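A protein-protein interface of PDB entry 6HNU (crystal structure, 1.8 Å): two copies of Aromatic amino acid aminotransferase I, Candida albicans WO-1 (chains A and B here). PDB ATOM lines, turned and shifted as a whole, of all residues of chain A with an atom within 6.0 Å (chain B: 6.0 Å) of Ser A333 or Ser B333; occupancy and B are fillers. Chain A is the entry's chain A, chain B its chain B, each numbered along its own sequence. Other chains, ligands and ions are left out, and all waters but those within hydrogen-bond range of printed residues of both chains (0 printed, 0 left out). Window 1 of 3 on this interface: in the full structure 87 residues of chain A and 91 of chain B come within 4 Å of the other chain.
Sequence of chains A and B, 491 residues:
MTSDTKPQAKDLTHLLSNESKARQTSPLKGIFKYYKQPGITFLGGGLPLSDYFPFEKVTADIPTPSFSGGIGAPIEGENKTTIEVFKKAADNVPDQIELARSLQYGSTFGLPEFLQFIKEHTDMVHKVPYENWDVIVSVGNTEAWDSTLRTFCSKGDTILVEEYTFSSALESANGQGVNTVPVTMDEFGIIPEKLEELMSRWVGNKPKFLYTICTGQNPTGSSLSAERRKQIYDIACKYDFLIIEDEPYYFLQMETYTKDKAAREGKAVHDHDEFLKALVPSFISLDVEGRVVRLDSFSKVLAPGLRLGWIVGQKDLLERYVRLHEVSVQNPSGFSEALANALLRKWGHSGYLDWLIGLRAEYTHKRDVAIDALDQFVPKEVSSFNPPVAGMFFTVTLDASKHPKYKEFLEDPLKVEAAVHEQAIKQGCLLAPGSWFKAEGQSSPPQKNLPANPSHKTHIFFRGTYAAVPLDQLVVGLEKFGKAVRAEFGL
Among the printed residues, merely in contact across the chains: Gly A305 with Ser B333 (3.6 Å), Leu A306 with Phe B335 (3.5 Å), Arg A307 with Asn B331 (3.2 Å), Arg A307 with Pro B332 (3.7 Å), Arg A307 with Ser B333 (3.8 Å), Asn A331 with Arg B307 (3.1 Å), Pro A332 with Arg B307 (3.6 Å), Ser A333 with Gly B305 (3.4 Å), Ser A333 with Arg B307 (3.6 Å), Ser A333 with Ser B333 (3.3 Å), Phe A335 with Leu B306 (3.8 Å), Phe A335 with Ser B336 (3.8 Å) and Ser A336 with Phe B335 (3.8 Å).
OG of Ser A333 is in hydrogen-bond range of OG of Ser B336, at 2.7 Å.
The side-chain hydroxyl of Ser A336 lies within hydrogen-bond range of the side-chain hydroxyl of Ser B333 (2.8 Å).
The backbone NH (N) of Gly A334 lies within hydrogen-bond range of the backbone carbonyl oxygen (O) of Gly B305, at 2.8 Å.
The backbone carbonyl oxygen (O) of Gly A305 is in hydrogen-bond range of the backbone NH (N) of Gly B334, at 2.8 Å.
Gly A305 touches Ser B333, and with the chains exchanged Ser A333 touches Gly B305.
Leu A306 touches Phe B335, and with the chains exchanged Phe A335 touches Leu B306.
Arg A307 touches Pro B332, and with the chains exchanged Pro A332 touches Arg B307.
Ser B333 touches its own counterpart, Ser A333.
Of the 17 pairs that touch across the chains among the printed residues, 17 have their exchanged pair printed and touching as well.
O of Val B139 is in hydrogen-bond range of NH2 of Arg B307, 3.4 Å away.
The backbone NH (N) of Ser A336 is in hydrogen-bond range of the side-chain hydroxyl (OG) of Ser A333 (3.1 Å).
The backbone NH of Ser B336 lies within hydrogen-bond range of the side-chain hydroxyl of Ser B333, at 3.1 Å.
The backbone carbonyl oxygen (O) of Leu A306 sits at hydrogen-bond distance from the side-chain hydroxyl (OG) of Ser A336 (2.5 Å).
The backbone NH (N) of Phe A335 sits at hydrogen-bond distance from the side-chain hydroxyl (OG) of Ser A333 (3.1 Å).
O of Leu B306 sits at hydrogen-bond distance from OG of Ser B336.
Hydrophobic or aromatic side chains of chain A within 4 Å of the printed part of chain B: Leu A306 and Phe A335.
Among the printed residues, 17 pairs touch across the chains.
Among the printed residues, no Asp or Glu carboxylate lies within 4 Å of a Lys or Arg side-chain nitrogen of the other chain.
Printed residues of chain B within 4 Å of Ser A333: Gly B305 (3.4 Å), Arg B307 (3.6 Å), Ser B333 (3.3 Å) and Ser B336 (2.7 Å).
Of the printed residues of chain B, Asn A331 touches Arg B307.
Of the printed residues of chain B, Arg A307 touches Asn B331 (3.2 Å), Pro B332 (3.7 Å) and Ser B333 (3.8 Å).
Printed residues of chain B within 4 Å of Gly A305: Ser B333 (3.6 Å) and Gly B334 (2.8 Å).
Printed residues of chain A within 4 Å of Ser B336: Ser A333 (2.7 Å) and Phe A335 (3.8 Å).
Leu B308 touches none of the printed residues of chain A.
Ser A102 touches none of the printed residues of chain B.
The nearest printed residue of chain B that does not touch Ser A333 is Leu B306 (4.02 Å).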
ATOM      1  N   SER A 102       3.201  26.839 -38.034  1.00  0.00           N
ATOM      2  CA  SER A 102       2.902  26.797 -36.580  1.00  0.00           C
ATOM      3  C   SER A 102       3.857  27.724 -35.816  1.00  0.00           C
ATOM      4  O   SER A 102       3.453  28.186 -34.704  1.00  0.00           O
ATOM      5  CB  SER A 102       2.846  25.410 -36.031  1.00  0.00           C
ATOM      6  OG  SER A 102       4.007  24.673 -36.328  1.00  0.00           O
ATOM      7  N   VAL A 139      -4.653  29.779 -23.663  1.00  0.00           N
ATOM      8  CA  VAL A 139      -3.384  29.237 -23.122  1.00  0.00           C
ATOM      9  C   VAL A 139      -3.661  28.613 -21.761  1.00  0.00           C
ATOM     10  O   VAL A 139      -2.760  28.610 -20.923  1.00  0.00           O
ATOM     11  CB  VAL A 139      -2.276  30.301 -23.116  1.00  0.00           C
ATOM     12  CG1 VAL A 139      -1.958  30.733 -24.546  1.00  0.00           C
ATOM     13  CG2 VAL A 139      -2.624  31.498 -22.262  1.00  0.00           C
ATOM     14  N   GLY A 305       1.797  21.733 -18.650  1.00  0.00           N
ATOM     15  CA  GLY A 305       2.796  22.478 -19.415  1.00  0.00           C
ATOM     16  C   GLY A 305       2.425  22.712 -20.860  1.00  0.00           C
ATOM     17  O   GLY A 305       3.124  23.483 -21.498  1.00  0.00           O
ATOM     18  N   LEU A 306       1.361  22.095 -21.387  1.00  0.00           N
ATOM     19  CA  LEU A 306       0.874  22.419 -22.750  1.00  0.00           C
ATOM     20  C   LEU A 306       0.533  23.919 -22.830  1.00  0.00           C
ATOM     21  O   LEU A 306       0.811  24.562 -23.859  1.00  0.00           O
ATOM     22  CB  LEU A 306      -0.353  21.547 -23.074  1.00  0.00           C
ATOM     23  CG  LEU A 306      -0.028  20.246 -23.810  1.00  0.00           C
ATOM     24  CD1 LEU A 306       0.880  19.395 -22.960  1.00  0.00           C
ATOM     25  CD2 LEU A 306      -1.275  19.463 -24.192  1.00  0.00           C
ATOM     26  N   ARG A 307       0.000  24.484 -21.747  1.00  0.00           N
ATOM     27  CA  ARG A 307      -0.573  25.862 -21.752  1.00  0.00           C
ATOM     28  C   ARG A 307      -1.446  25.975 -22.998  1.00  0.00           C
ATOM     29  O   ARG A 307      -1.256  26.870 -23.800  1.00  0.00           O
ATOM     30  CB  ARG A 307       0.491  26.951 -21.697  1.00  0.00           C
ATOM     31  CG  ARG A 307       1.304  26.934 -20.416  1.00  0.00           C
ATOM     32  CD  ARG A 307       0.499  27.388 -19.197  1.00  0.00           C
ATOM     33  NE  ARG A 307      -0.094  26.244 -18.511  1.00  0.00           N
ATOM     34  CZ  ARG A 307      -1.261  26.222 -17.880  1.00  0.00           C
ATOM     35  NH1 ARG A 307      -1.656  25.106 -17.295  1.00  0.00           N
ATOM     36  NH2 ARG A 307      -2.037  27.297 -17.843  1.00  0.00           N
ATOM     37  N   LEU A 308      -2.408  25.077 -23.097  1.00  0.00           N
ATOM     38  CA  LEU A 308      -3.305  25.012 -24.267  1.00  0.00           C
ATOM     39  C   LEU A 308      -4.671  24.561 -23.793  1.00  0.00           C
ATOM     40  O   LEU A 308      -4.773  23.595 -23.028  1.00  0.00           O
ATOM     41  CB  LEU A 308      -2.708  24.050 -25.300  1.00  0.00           C
ATOM     42  CG  LEU A 308      -3.516  23.906 -26.584  1.00  0.00           C
ATOM     43  CD1 LEU A 308      -3.636  25.233 -27.294  1.00  0.00           C
ATOM     44  CD2 LEU A 308      -2.886  22.856 -27.494  1.00  0.00           C
ATOM     45  N   ASN A 331      -1.264  34.271 -28.865  1.00  0.00           N
ATOM     46  CA  ASN A 331      -1.554  32.891 -29.310  1.00  0.00           C
ATOM     47  C   ASN A 331      -0.836  31.906 -28.395  1.00  0.00           C
ATOM     48  O   ASN A 331       0.158  32.252 -27.757  1.00  0.00           O
ATOM     49  CB  ASN A 331      -1.121  32.655 -30.764  1.00  0.00           C
ATOM     50  CG  ASN A 331      -2.302  32.586 -31.705  1.00  0.00           C
ATOM     51  OD1 ASN A 331      -3.416  32.190 -31.320  1.00  0.00           O
ATOM     52  ND2 ASN A 331      -2.063  32.959 -32.944  1.00  0.00           N
ATOM     53  N   PRO A 332      -1.327  30.660 -28.318  1.00  0.00           N
ATOM     54  CA  PRO A 332      -0.587  29.602 -27.647  1.00  0.00           C
ATOM     55  C   PRO A 332       0.706  29.367 -28.423  1.00  0.00           C
ATOM     56  O   PRO A 332       0.785  29.712 -29.605  1.00  0.00           O
ATOM     57  CB  PRO A 332      -1.512  28.373 -27.675  1.00  0.00           C
ATOM     58  CG  PRO A 332      -2.863  28.887 -28.157  1.00  0.00           C
ATOM     59  CD  PRO A 332      -2.590  30.180 -28.902  1.00  0.00           C
ATOM     60  N   SER A 333       1.685  28.811 -27.729  1.00  0.00           N
ATOM     61  CA  SER A 333       2.921  28.243 -28.296  1.00  0.00           C
ATOM     62  C   SER A 333       2.546  27.383 -29.495  1.00  0.00           C
ATOM     63  O   SER A 333       1.654  26.513 -29.366  1.00  0.00           O
ATOM     64  CB  SER A 333       3.631  27.431 -27.272  1.00  0.00           C
ATOM     65  OG  SER A 333       4.571  26.531 -27.868  1.00  0.00           O
ATOM     66  N   GLY A 334       3.224  27.625 -30.609  1.00  0.00           N
ATOM     67  CA  GLY A 334       3.064  26.837 -31.833  1.00  0.00           C
ATOM     68  C   GLY A 334       3.603  25.437 -31.633  1.00  0.00           C
ATOM     69  O   GLY A 334       3.084  24.508 -32.323  1.00  0.00           O
ATOM     70  N   PHE A 335       4.579  25.250 -30.735  1.00  0.00           N
ATOM     71  CA  PHE A 335       5.054  23.894 -30.341  1.00  0.00           C
ATOM     72  C   PHE A 335       3.901  23.156 -29.655  1.00  0.00           C
ATOM     73  O   PHE A 335       3.580  22.019 -30.026  1.00  0.00           O
ATOM     74  CB  PHE A 335       6.292  23.930 -29.438  1.00  0.00           C
ATOM     75  CG  PHE A 335       7.542  24.321 -30.172  1.00  0.00           C
ATOM     76  CD1 PHE A 335       8.040  23.525 -31.195  1.00  0.00           C
ATOM     77  CD2 PHE A 335       8.212  25.483 -29.859  1.00  0.00           C
ATOM     78  CE1 PHE A 335       9.192  23.894 -31.882  1.00  0.00           C
ATOM     79  CE2 PHE A 335       9.369  25.845 -30.540  1.00  0.00           C
ATOM     80  CZ  PHE A 335       9.854  25.041 -31.554  1.00  0.00           C
ATOM     81  N   SER A 336       3.266  23.797 -28.680  1.00  0.00           N
ATOM     82  CA  SER A 336       2.139  23.184 -27.938  1.00  0.00           C
ATOM     83  C   SER A 336       1.030  22.821 -28.928  1.00  0.00           C
ATOM     84  O   SER A 336       0.497  21.704 -28.856  1.00  0.00           O
ATOM     85  CB  SER A 336       1.613  24.083 -26.861  1.00  0.00           C
ATOM     86  OG  SER A 336       2.406  24.000 -25.691  1.00  0.00           O
ATOM     87  N   GLU A 337       0.661  23.764 -29.782  1.00  0.00           N
ATOM     88  CA  GLU A 337      -0.488  23.584 -30.688  1.00  0.00           C
ATOM     89  C   GLU A 337      -0.142  22.514 -31.737  1.00  0.00           C
ATOM     90  O   GLU A 337      -0.990  21.644 -31.955  1.00  0.00           O
ATOM     91  CB  GLU A 337      -0.908  24.914 -31.286  1.00  0.00           C
ATOM     92  CG  GLU A 337      -2.357  24.889 -31.658  1.00  0.00           C
ATOM     93  CD  GLU A 337      -2.966  26.245 -31.928  1.00  0.00           C
ATOM     94  OE1 GLU A 337      -2.405  27.250 -31.469  1.00  0.00           O
ATOM     95  OE2 GLU A 337      -3.994  26.249 -32.612  1.00  0.00           O
ATOM     96  N   ALA A 338       1.044  22.545 -32.329  1.00  0.00           N
ATOM     97  CA  ALA A 338       1.446  21.586 -33.390  1.00  0.00           C
ATOM     98  C   ALA A 338       1.587  20.172 -32.813  1.00  0.00           C
ATOM     99  O   ALA A 338       1.116  19.204 -33.449  1.00  0.00           O
ATOM    100  CB  ALA A 338       2.717  22.048 -34.057  1.00  0.00           C
ATOM    101  N   SER B 102       9.184  20.260 -16.794  1.00  0.00           N
ATOM    102  CA  SER B 102       8.780  21.375 -17.702  1.00  0.00           C
ATOM    103  C   SER B 102       7.283  21.291 -18.068  1.00  0.00           C
ATOM    104  O   SER B 102       6.705  22.334 -18.392  1.00  0.00           O
ATOM    105  CB  SER B 102       9.685  21.452 -18.937  1.00  0.00           C
ATOM    106  OG  SER B 102       9.917  20.169 -19.505  1.00  0.00           O
ATOM    107  N   VAL B 139       5.235  35.423 -22.063  1.00  0.00           N
ATOM    108  CA  VAL B 139       4.848  34.647 -23.276  1.00  0.00           C
ATOM    109  C   VAL B 139       4.962  35.546 -24.506  1.00  0.00           C
ATOM    110  O   VAL B 139       4.253  35.305 -25.528  1.00  0.00           O
ATOM    111  CB  VAL B 139       3.464  33.990 -23.087  1.00  0.00           C
ATOM    112  CG1 VAL B 139       3.508  33.030 -21.917  1.00  0.00           C
ATOM    113  CG2 VAL B 139       2.354  34.991 -22.868  1.00  0.00           C
ATOM    114  N   GLY B 305       6.359  31.750 -32.911  1.00  0.00           N
ATOM    115  CA  GLY B 305       5.533  30.675 -32.324  1.00  0.00           C
ATOM    116  C   GLY B 305       6.094  30.148 -31.011  1.00  0.00           C
ATOM    117  O   GLY B 305       5.412  29.346 -30.379  1.00  0.00           O
ATOM    118  N   LEU B 306       7.321  30.501 -30.624  1.00  0.00           N
ATOM    119  CA  LEU B 306       7.839  30.150 -29.276  1.00  0.00           C
ATOM    120  C   LEU B 306       6.880  30.710 -28.221  1.00  0.00           C
ATOM    121  O   LEU B 306       6.689  30.038 -27.181  1.00  0.00           O
ATOM    122  CB  LEU B 306       9.255  30.702 -29.070  1.00  0.00           C
ATOM    123  CG  LEU B 306      10.393  29.745 -29.431  1.00  0.00           C
ATOM    124  CD1 LEU B 306      11.672  30.510 -29.728  1.00  0.00           C
ATOM    125  CD2 LEU B 306      10.637  28.711 -28.336  1.00  0.00           C
ATOM    126  N   ARG B 307       6.363  31.912 -28.447  1.00  0.00           N
ATOM    127  CA  ARG B 307       5.502  32.544 -27.411  1.00  0.00           C
ATOM    128  C   ARG B 307       6.315  32.526 -26.105  1.00  0.00           C
ATOM    129  O   ARG B 307       5.858  32.022 -25.118  1.00  0.00           O
ATOM    130  CB  ARG B 307       4.164  31.822 -27.276  1.00  0.00           C
ATOM    131  CG  ARG B 307       3.183  32.061 -28.414  1.00  0.00           C
ATOM    132  CD  ARG B 307       2.853  33.525 -28.617  1.00  0.00           C
ATOM    133  NE  ARG B 307       3.758  34.138 -29.562  1.00  0.00           N
ATOM    134  CZ  ARG B 307       4.082  35.412 -29.615  1.00  0.00           C
ATOM    135  NH1 ARG B 307       4.919  35.817 -30.541  1.00  0.00           N
ATOM    136  NH2 ARG B 307       3.608  36.273 -28.730  1.00  0.00           N
ATOM    137  N   LEU B 308       7.508  33.098 -26.166  1.00  0.00           N
ATOM    138  CA  LEU B 308       8.461  33.093 -25.050  1.00  0.00           C
ATOM    139  C   LEU B 308       9.284  34.367 -25.124  1.00  0.00           C
ATOM    140  O   LEU B 308       9.891  34.679 -26.172  1.00  0.00           O
ATOM    141  CB  LEU B 308       9.377  31.875 -25.145  1.00  0.00           C
ATOM    142  CG  LEU B 308      10.333  31.648 -23.978  1.00  0.00           C
ATOM    143  CD1 LEU B 308       9.603  31.475 -22.646  1.00  0.00           C
ATOM    144  CD2 LEU B 308      11.187  30.407 -24.247  1.00  0.00           C
ATOM    145  N   ASN B 331       2.212  30.669 -17.061  1.00  0.00           N
ATOM    146  CA  ASN B 331       3.597  30.341 -17.445  1.00  0.00           C
ATOM    147  C   ASN B 331       3.634  30.133 -18.943  1.00  0.00           C
ATOM    148  O   ASN B 331       2.609  29.822 -19.504  1.00  0.00           O
ATOM    149  CB  ASN B 331       4.087  29.067 -16.752  1.00  0.00           C
ATOM    150  CG  ASN B 331       5.005  29.389 -15.594  1.00  0.00           C
ATOM    151  OD1 ASN B 331       5.795  30.339 -15.682  1.00  0.00           O
ATOM    152  ND2 ASN B 331       4.932  28.594 -14.529  1.00  0.00           N
ATOM    153  N   PRO B 332       4.789  30.304 -19.613  1.00  0.00           N
ATOM    154  CA  PRO B 332       4.916  29.889 -21.001  1.00  0.00           C
ATOM    155  C   PRO B 332       4.724  28.385 -21.134  1.00  0.00           C
ATOM    156  O   PRO B 332       4.921  27.648 -20.132  1.00  0.00           O
ATOM    157  CB  PRO B 332       6.378  30.228 -21.337  1.00  0.00           C
ATOM    158  CG  PRO B 332       6.765  31.258 -20.312  1.00  0.00           C
ATOM    159  CD  PRO B 332       6.050  30.816 -19.067  1.00  0.00           C
ATOM    160  N   SER B 333       4.425  27.940 -22.360  1.00  0.00           N
ATOM    161  CA  SER B 333       4.475  26.527 -22.769  1.00  0.00           C
ATOM    162  C   SER B 333       5.768  25.876 -22.255  1.00  0.00           C
ATOM    163  O   SER B 333       6.907  26.400 -22.540  1.00  0.00           O
ATOM    164  CB  SER B 333       4.426  26.376 -24.257  1.00  0.00           C
ATOM    165  OG  SER B 333       4.753  25.038 -24.637  1.00  0.00           O
ATOM    166  N   GLY B 334       5.608  24.724 -21.614  1.00  0.00           N
ATOM    167  CA  GLY B 334       6.737  23.920 -21.114  1.00  0.00           C
ATOM    168  C   GLY B 334       7.518  23.399 -22.308  1.00  0.00           C
ATOM    169  O   GLY B 334       8.735  23.221 -22.219  1.00  0.00           O
ATOM    170  N   PHE B 335       6.820  23.114 -23.412  1.00  0.00           N
ATOM    171  CA  PHE B 335       7.494  22.681 -24.656  1.00  0.00           C
ATOM    172  C   PHE B 335       8.348  23.836 -25.157  1.00  0.00           C
ATOM    173  O   PHE B 335       9.503  23.602 -25.488  1.00  0.00           O
ATOM    174  CB  PHE B 335       6.516  22.188 -25.721  1.00  0.00           C
ATOM    175  CG  PHE B 335       5.826  20.886 -25.391  1.00  0.00           C
ATOM    176  CD1 PHE B 335       6.552  19.708 -25.313  1.00  0.00           C
ATOM    177  CD2 PHE B 335       4.453  20.829 -25.229  1.00  0.00           C
ATOM    178  CE1 PHE B 335       5.910  18.509 -25.010  1.00  0.00           C
ATOM    179  CE2 PHE B 335       3.812  19.638 -24.921  1.00  0.00           C
ATOM    180  CZ  PHE B 335       4.549  18.473 -24.836  1.00  0.00           C
ATOM    181  N   SER B 336       7.818  25.070 -25.270  1.00  0.00           N
ATOM    182  CA  SER B 336       8.638  26.218 -25.751  1.00  0.00           C
ATOM    183  C   SER B 336       9.857  26.398 -24.822  1.00  0.00           C
ATOM    184  O   SER B 336      11.000  26.593 -25.298  1.00  0.00           O
ATOM    185  CB  SER B 336       7.810  27.498 -25.811  1.00  0.00           C
ATOM    186  OG  SER B 336       6.864  27.411 -26.852  1.00  0.00           O
ATOM    187  N   GLU B 337       9.648  26.372 -23.513  1.00  0.00           N
ATOM    188  CA  GLU B 337      10.733  26.784 -22.582  1.00  0.00           C
ATOM    189  C   GLU B 337      11.796  25.678 -22.526  1.00  0.00           C
ATOM    190  O   GLU B 337      13.003  25.994 -22.434  1.00  0.00           O
ATOM    191  CB  GLU B 337      10.150  27.091 -21.209  1.00  0.00           C
ATOM    192  CG  GLU B 337      10.986  28.087 -20.466  1.00  0.00           C
ATOM    193  CD  GLU B 337      10.414  28.540 -19.137  1.00  0.00           C
ATOM    194  OE1 GLU B 337       9.184  28.602 -19.005  1.00  0.00           O
ATOM    195  OE2 GLU B 337      11.225  28.803 -18.248  1.00  0.00           O
ATOM    196  N   ALA B 338      11.358  24.416 -22.546  1.00  0.00           N
ATOM    197  CA  ALA B 338      12.274  23.250 -22.531  1.00  0.00           C
ATOM    198  C   ALA B 338      13.055  23.197 -23.853  1.00  0.00           C
ATOM    199  O   ALA B 338      14.299  22.990 -23.802  1.00  0.00           O
ATOM    200  CB  ALA B 338      11.512  21.976 -22.283  1.00  0.00           C
